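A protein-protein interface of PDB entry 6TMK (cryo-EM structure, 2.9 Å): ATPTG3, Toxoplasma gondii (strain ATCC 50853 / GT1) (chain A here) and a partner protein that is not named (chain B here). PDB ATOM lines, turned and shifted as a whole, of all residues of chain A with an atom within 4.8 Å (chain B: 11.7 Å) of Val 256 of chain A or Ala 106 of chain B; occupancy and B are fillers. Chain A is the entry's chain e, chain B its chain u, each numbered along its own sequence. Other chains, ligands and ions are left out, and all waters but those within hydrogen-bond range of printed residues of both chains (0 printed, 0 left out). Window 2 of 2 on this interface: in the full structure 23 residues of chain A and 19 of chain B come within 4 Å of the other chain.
Printed residues of chain A that touch a printed residue of chain B: Val 251, Pro 252, Thr 253, Gly 254, Thr 255, Val 256 and Pro 258.
Hydrophobic or aromatic side chains of chain A within 4 Å of the printed part of chain B: Val 251, Val 256 and Pro 258.
Of the 16 printed residues of chain B, 5 touch a printed residue of chain A.
Hydrophobic or aromatic side chains of chain B within 4 Å of the printed part of chain A: Val 105, Ala 106 and Tyr 108.
Among the printed residues, no Asp or Glu carboxylate lies within 4 Å of a Lys or Arg side-chain nitrogen of the other chain.
The backbone carbonyl oxygen (O) of Ala 106 of chain B lies within hydrogen-bond range of the backbone NH (N) of Thr 255 of chain A.
O of Ala 106 of chain B sits at hydrogen-bond distance from N of Gly 254 of chain A, 3.1 Å away.
N of Gly 254 of chain A is in hydrogen-bond range of O of Tyr 108 of chain B, at 2.8 Å.
The backbone carbonyl oxygen (O) of Pro 252 of chain A sits at hydrogen-bond distance from the side-chain hydroxyl (OG1) of Thr 255 of chain A, 3.3 Å away.
Among the printed residues, merely in contact across the chains: Pro 252 of chain A with Ala 106 of chain B (3.3 Å), Thr 253 of chain A with Val 105 of chain B (3.3 Å), Thr 253 of chain A with Tyr 108 of chain B (3.4 Å), Val 251 of chain A with Ala 106 of chain B (3.6 Å), Val 256 of chain A with Ala 106 of chain B (3.6 Å), Pro 258 of chain A with Glu 107 of chain B (3.7 Å), Pro 252 of chain A with Val 105 of chain B (3.8 Å), Val 256 of chain A with Glu 107 of chain B (3.9 Å), Val 251 of chain A with Val 105 of chain B (3.96 Å) and Val 251 of chain A with Ala 102 of chain B (3.99 Å).
Of chain B, only Val 105 (3.3 Å) and Tyr 108 (3.4 Å) come within 4 Å of Thr 253 of chain A.
Of chain B, only Ala 106 (3.1 Å) and Tyr 108 (2.8 Å) come within 4 Å of Gly 254 of chain A.
Thr 255 of chain A touches just one residue of chain B: Ala 106.
Of chain B, only Ala 106 and Glu 107 come within 4 Å of Val 256 of chain A.
No residue of chain B comes within 4 Å of Ser 257 of chain A.
Of chain B, only Glu 107 comes within 4 Å of Pro 258 of chain A.
Printed residues of chain A within 4 Å of Ala 102 of chain B: Val 251 (3.99 Å).
Of the printed residues of chain A, Val 105 of chain B touches Val 251 (3.96 Å), Pro 252 (3.8 Å) and Thr 253 (3.3 Å).
Of chain A, only Val 251, Pro 252, Gly 254, Thr 255 and Val 256 come within 4 Å of Ala 106 of chain B.
Printed residues of chain A within 4 Å of Glu 107 of chain B: Val 256 (3.9 Å) and Pro 258 (3.7 Å).
Printed residues of chain A within 4 Å of Tyr 108 of chain B: Thr 253 (3.4 Å) and Gly 254 (2.8 Å).
Val 111 of chain B touches none of the printed residues of chain A.
The nearest residue of chain B that does not touch Val 256 of chain A is Tyr 108 of chain B (5.7 Å).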
ATOM      1  N   VAL A 251      15.854  36.396  22.359  1.00  0.00           N
ATOM      2  CA  VAL A 251      14.716  35.880  23.112  1.00  0.00           C
ATOM      3  C   VAL A 251      15.234  35.081  24.299  1.00  0.00           C
ATOM      4  O   VAL A 251      16.231  34.359  24.164  1.00  0.00           O
ATOM      5  CB  VAL A 251      13.808  35.013  22.231  1.00  0.00           C
ATOM      6  CG1 VAL A 251      12.641  34.516  23.019  1.00  0.00           C
ATOM      7  CG2 VAL A 251      13.321  35.783  21.052  1.00  0.00           C
ATOM      8  N   PRO A 252      14.602  35.166  25.465  1.00  0.00           N
ATOM      9  CA  PRO A 252      14.937  34.251  26.553  1.00  0.00           C
ATOM     10  C   PRO A 252      14.122  32.969  26.523  1.00  0.00           C
ATOM     11  O   PRO A 252      12.959  32.938  26.121  1.00  0.00           O
ATOM     12  CB  PRO A 252      14.601  35.084  27.795  1.00  0.00           C
ATOM     13  CG  PRO A 252      13.475  35.901  27.364  1.00  0.00           C
ATOM     14  CD  PRO A 252      13.738  36.257  25.937  1.00  0.00           C
ATOM     15  N   THR A 253      14.762  31.898  26.971  1.00  0.00           N
ATOM     16  CA  THR A 253      14.165  30.575  26.951  1.00  0.00           C
ATOM     17  C   THR A 253      13.362  30.316  28.218  1.00  0.00           C
ATOM     18  O   THR A 253      13.698  30.796  29.303  1.00  0.00           O
ATOM     19  CB  THR A 253      15.239  29.502  26.801  1.00  0.00           C
ATOM     20  OG1 THR A 253      16.234  29.665  27.816  1.00  0.00           O
ATOM     21  CG2 THR A 253      15.887  29.593  25.456  1.00  0.00           C
ATOM     22  N   GLY A 254      12.291  29.543  28.065  1.00  0.00           N
ATOM     23  CA  GLY A 254      11.519  29.092  29.200  1.00  0.00           C
ATOM     24  C   GLY A 254      10.630  30.132  29.826  1.00  0.00           C
ATOM     25  O   GLY A 254      10.218  29.963  30.977  1.00  0.00           O
ATOM     26  N   THR A 255      10.308  31.199  29.104  1.00  0.00           N
ATOM     27  CA  THR A 255       9.522  32.296  29.637  1.00  0.00           C
ATOM     28  C   THR A 255       8.072  32.228  29.199  1.00  0.00           C
ATOM     29  O   THR A 255       7.301  33.147  29.487  1.00  0.00           O
ATOM     30  CB  THR A 255      10.131  33.630  29.210  1.00  0.00           C
ATOM     31  OG1 THR A 255      10.248  33.661  27.785  1.00  0.00           O
ATOM     32  CG2 THR A 255      11.480  33.829  29.838  1.00  0.00           C
ATOM     33  N   VAL A 256       7.686  31.159  28.513  1.00  0.00           N
ATOM     34  CA  VAL A 256       6.381  31.083  27.873  1.00  0.00           C
ATOM     35  C   VAL A 256       5.916  29.634  27.895  1.00  0.00           C
ATOM     36  O   VAL A 256       6.685  28.714  27.610  1.00  0.00           O
ATOM     37  CB  VAL A 256       6.443  31.638  26.436  1.00  0.00           C
ATOM     38  CG1 VAL A 256       5.267  31.174  25.638  1.00  0.00           C
ATOM     39  CG2 VAL A 256       6.492  33.139  26.463  1.00  0.00           C
ATOM     40  N   SER A 257       4.647  29.443  28.241  1.00  0.00           N
ATOM     41  CA  SER A 257       3.988  28.138  28.229  1.00  0.00           C
ATOM     42  C   SER A 257       2.644  28.322  27.543  1.00  0.00           C
ATOM     43  O   SER A 257       1.617  28.502  28.210  1.00  0.00           O
ATOM     44  CB  SER A 257       3.836  27.574  29.640  1.00  0.00           C
ATOM     45  OG  SER A 257       5.096  27.250  30.197  1.00  0.00           O
ATOM     46  N   PRO A 258       2.606  28.283  26.209  1.00  0.00           N
ATOM     47  CA  PRO A 258       1.368  28.670  25.522  1.00  0.00           C
ATOM     48  C   PRO A 258       0.225  27.700  25.729  1.00  0.00           C
ATOM     49  O   PRO A 258      -0.936  28.119  25.658  1.00  0.00           O
ATOM     50  CB  PRO A 258       1.790  28.721  24.046  1.00  0.00           C
ATOM     51  CG  PRO A 258       3.270  28.764  24.069  1.00  0.00           C
ATOM     52  CD  PRO A 258       3.661  27.951  25.245  1.00  0.00           C
ATOM     53  N   ALA B  98      12.698  32.464   9.320  1.00  0.00           N
ATOM     54  CA  ALA B  98      13.629  32.367  10.435  1.00  0.00           C
ATOM     55  C   ALA B  98      13.094  33.088  11.662  1.00  0.00           C
ATOM     56  O   ALA B  98      13.270  32.620  12.789  1.00  0.00           O
ATOM     57  CB  ALA B  98      14.982  32.934  10.032  1.00  0.00           C
ATOM     58  N   GLY B  99      12.438  34.227  11.462  1.00  0.00           N
ATOM     59  CA  GLY B  99      11.825  34.921  12.582  1.00  0.00           C
ATOM     60  C   GLY B  99      10.688  34.127  13.191  1.00  0.00           C
ATOM     61  O   GLY B  99      10.512  34.098  14.417  1.00  0.00           O
ATOM     62  N   HIS B 100       9.902  33.470  12.345  1.00  0.00           N
ATOM     63  CA  HIS B 100       8.871  32.581  12.859  1.00  0.00           C
ATOM     64  C   HIS B 100       9.473  31.511  13.757  1.00  0.00           C
ATOM     65  O   HIS B 100       8.938  31.218  14.831  1.00  0.00           O
ATOM     66  CB  HIS B 100       8.120  31.926  11.709  1.00  0.00           C
ATOM     67  CG  HIS B 100       6.948  31.110  12.147  1.00  0.00           C
ATOM     68  ND1 HIS B 100       7.088  29.952  12.879  1.00  0.00           N
ATOM     69  CD2 HIS B 100       5.621  31.268  11.941  1.00  0.00           C
ATOM     70  CE1 HIS B 100       5.895  29.443  13.124  1.00  0.00           C
ATOM     71  NE2 HIS B 100       4.989  30.220  12.565  1.00  0.00           N
ATOM     72  N   ILE B 101      10.588  30.915  13.338  1.00  0.00           N
ATOM     73  CA  ILE B 101      11.210  29.893  14.176  1.00  0.00           C
ATOM     74  C   ILE B 101      11.816  30.508  15.430  1.00  0.00           C
ATOM     75  O   ILE B 101      11.833  29.875  16.491  1.00  0.00           O
ATOM     76  CB  ILE B 101      12.257  29.094  13.386  1.00  0.00           C
ATOM     77  CG1 ILE B 101      11.577  28.219  12.344  1.00  0.00           C
ATOM     78  CG2 ILE B 101      13.091  28.257  14.320  1.00  0.00           C
ATOM     79  CD1 ILE B 101      12.489  27.746  11.284  1.00  0.00           C
ATOM     80  N   ALA B 102      12.335  31.729  15.335  1.00  0.00           N
ATOM     81  CA  ALA B 102      12.913  32.382  16.499  1.00  0.00           C
ATOM     82  C   ALA B 102      11.861  32.656  17.556  1.00  0.00           C
ATOM     83  O   ALA B 102      12.180  32.736  18.746  1.00  0.00           O
ATOM     84  CB  ALA B 102      13.591  33.682  16.086  1.00  0.00           C
ATOM     85  N   SER B 103      10.604  32.808  17.145  1.00  0.00           N
ATOM     86  CA  SER B 103       9.539  32.978  18.124  1.00  0.00           C
ATOM     87  C   SER B 103       9.339  31.751  19.013  1.00  0.00           C
ATOM     88  O   SER B 103       8.645  31.856  20.028  1.00  0.00           O
ATOM     89  CB  SER B 103       8.230  33.331  17.417  1.00  0.00           C
ATOM     90  OG  SER B 103       7.735  32.253  16.651  1.00  0.00           O
ATOM     91  N   LEU B 104       9.921  30.602  18.669  1.00  0.00           N
ATOM     92  CA  LEU B 104       9.796  29.386  19.465  1.00  0.00           C
ATOM     93  C   LEU B 104      10.867  29.243  20.539  1.00  0.00           C
ATOM     94  O   LEU B 104      10.748  28.363  21.401  1.00  0.00           O
ATOM     95  CB  LEU B 104       9.866  28.161  18.558  1.00  0.00           C
ATOM     96  CG  LEU B 104       8.826  28.035  17.453  1.00  0.00           C
ATOM     97  CD1 LEU B 104       9.236  26.971  16.467  1.00  0.00           C
ATOM     98  CD2 LEU B 104       7.500  27.688  18.042  1.00  0.00           C
ATOM     99  N   VAL B 105      11.913  30.067  20.496  1.00  0.00           N
ATOM    100  CA  VAL B 105      12.967  29.983  21.497  1.00  0.00           C
ATOM    101  C   VAL B 105      12.431  30.337  22.873  1.00  0.00           C
ATOM    102  O   VAL B 105      12.968  29.888  23.891  1.00  0.00           O
ATOM    103  CB  VAL B 105      14.136  30.893  21.079  1.00  0.00           C
ATOM    104  CG1 VAL B 105      15.110  31.096  22.219  1.00  0.00           C
ATOM    105  CG2 VAL B 105      14.831  30.304  19.887  1.00  0.00           C
ATOM    106  N   ALA B 106      11.362  31.129  22.931  1.00  0.00           N
ATOM    107  CA  ALA B 106      10.736  31.426  24.211  1.00  0.00           C
ATOM    108  C   ALA B 106      10.019  30.208  24.771  1.00  0.00           C
ATOM    109  O   ALA B 106      10.021  29.985  25.986  1.00  0.00           O
ATOM    110  CB  ALA B 106       9.770  32.593  24.047  1.00  0.00           C
ATOM    111  N   GLU B 107       9.397  29.414  23.902  1.00  0.00           N
ATOM    112  CA  GLU B 107       8.733  28.199  24.347  1.00  0.00           C
ATOM    113  C   GLU B 107       9.738  27.129  24.736  1.00  0.00           C
ATOM    114  O   GLU B 107       9.460  26.307  25.615  1.00  0.00           O
ATOM    115  CB  GLU B 107       7.809  27.672  23.255  1.00  0.00           C
ATOM    116  CG  GLU B 107       6.749  28.646  22.823  1.00  0.00           C
ATOM    117  CD  GLU B 107       6.039  28.192  21.564  1.00  0.00           C
ATOM    118  OE1 GLU B 107       5.411  29.039  20.892  1.00  0.00           O
ATOM    119  OE2 GLU B 107       6.110  26.987  21.247  1.00  0.00           O
ATOM    120  N   TYR B 108      10.901  27.125  24.097  1.00  0.00           N
ATOM    121  CA  TYR B 108      11.919  26.135  24.412  1.00  0.00           C
ATOM    122  C   TYR B 108      12.315  26.215  25.878  1.00  0.00           C
ATOM    123  O   TYR B 108      12.672  27.280  26.386  1.00  0.00           O
ATOM    124  CB  TYR B 108      13.142  26.333  23.526  1.00  0.00           C
ATOM    125  CG  TYR B 108      14.289  25.413  23.859  1.00  0.00           C
ATOM    126  CD1 TYR B 108      14.185  24.052  23.664  1.00  0.00           C
ATOM    127  CD2 TYR B 108      15.471  25.905  24.375  1.00  0.00           C
ATOM    128  CE1 TYR B 108      15.214  23.212  23.968  1.00  0.00           C
ATOM    129  CE2 TYR B 108      16.509  25.068  24.680  1.00  0.00           C
ATOM    130  CZ  TYR B 108      16.377  23.720  24.474  1.00  0.00           C
ATOM    131  OH  TYR B 108      17.414  22.878  24.778  1.00  0.00           O
ATOM    132  N   ASP B 109      12.240  25.077  26.552  1.00  0.00           N
ATOM    133  CA  ASP B 109      12.632  24.941  27.951  1.00  0.00           C
ATOM    134  C   ASP B 109      13.715  23.881  28.055  1.00  0.00           C
ATOM    135  O   ASP B 109      13.415  22.682  27.906  1.00  0.00           O
ATOM    136  CB  ASP B 109      11.436  24.566  28.821  1.00  0.00           C
ATOM    137  CG  ASP B 109      11.704  24.768  30.295  1.00  0.00           C
ATOM    138  OD1 ASP B 109      10.755  24.639  31.095  1.00  0.00           O
ATOM    139  OD2 ASP B 109      12.862  25.064  30.653  1.00  0.00           O
ATOM    140  N   PRO B 110      14.978  24.246  28.293  1.00  0.00           N
ATOM    141  CA  PRO B 110      16.032  23.229  28.348  1.00  0.00           C
ATOM    142  C   PRO B 110      16.047  22.414  29.623  1.00  0.00           C
ATOM    143  O   PRO B 110      16.817  21.449  29.707  1.00  0.00           O
ATOM    144  CB  PRO B 110      17.305  24.065  28.221  1.00  0.00           C
ATOM    145  CG  PRO B 110      16.953  25.335  28.852  1.00  0.00           C
ATOM    146  CD  PRO B 110      15.537  25.598  28.443  1.00  0.00           C
ATOM    147  N   VAL B 111      15.229  22.762  30.613  1.00  0.00           N
ATOM    148  CA  VAL B 111      15.174  21.979  31.838  1.00  0.00           C
ATOM    149  C   VAL B 111      14.371  20.706  31.627  1.00  0.00           C
ATOM    150  O   VAL B 111      14.614  19.695  32.293  1.00  0.00           O
ATOM    151  CB  VAL B 111      14.587  22.824  32.978  1.00  0.00           C
ATOM    152  CG1 VAL B 111      14.432  21.995  34.222  1.00  0.00           C
ATOM    153  CG2 VAL B 111      15.466  24.014  33.244  1.00  0.00           C
ATOM    154  N   ALA B 112      13.413  20.731  30.703  1.00  0.00           N
ATOM    155  CA  ALA B 112      12.623  19.547  30.406  1.00  0.00           C
ATOM    156  C   ALA B 112      13.456  18.423  29.816  1.00  0.00           C
ATOM    157  O   ALA B 112      13.055  17.258  29.898  1.00  0.00           O
ATOM    158  CB  ALA B 112      11.508  19.915  29.443  1.00  0.00           C
ATOM    159  N   ARG B 125      22.320  24.521  26.214  1.00  0.00           N
ATOM    160  CA  ARG B 125      22.403  25.976  26.346  1.00  0.00           C
ATOM    161  C   ARG B 125      21.779  26.469  27.654  1.00  0.00           C
ATOM    162  O   ARG B 125      20.754  27.148  27.677  1.00  0.00           O
ATOM    163  CB  ARG B 125      21.763  26.662  25.138  1.00  0.00           C
ATOM    164  CG  ARG B 125      20.329  26.322  24.910  1.00  0.00           C
ATOM    165  CD  ARG B 125      19.737  27.190  23.837  1.00  0.00           C
ATOM    166  NE  ARG B 125      20.296  26.871  22.532  1.00  0.00           N
ATOM    167  CZ  ARG B 125      19.915  27.450  21.399  1.00  0.00           C
ATOM    168  NH1 ARG B 125      18.973  28.382  21.412  1.00  0.00           N
ATOM    169  NH2 ARG B 125      20.479  27.097  20.253  1.00  0.00           N
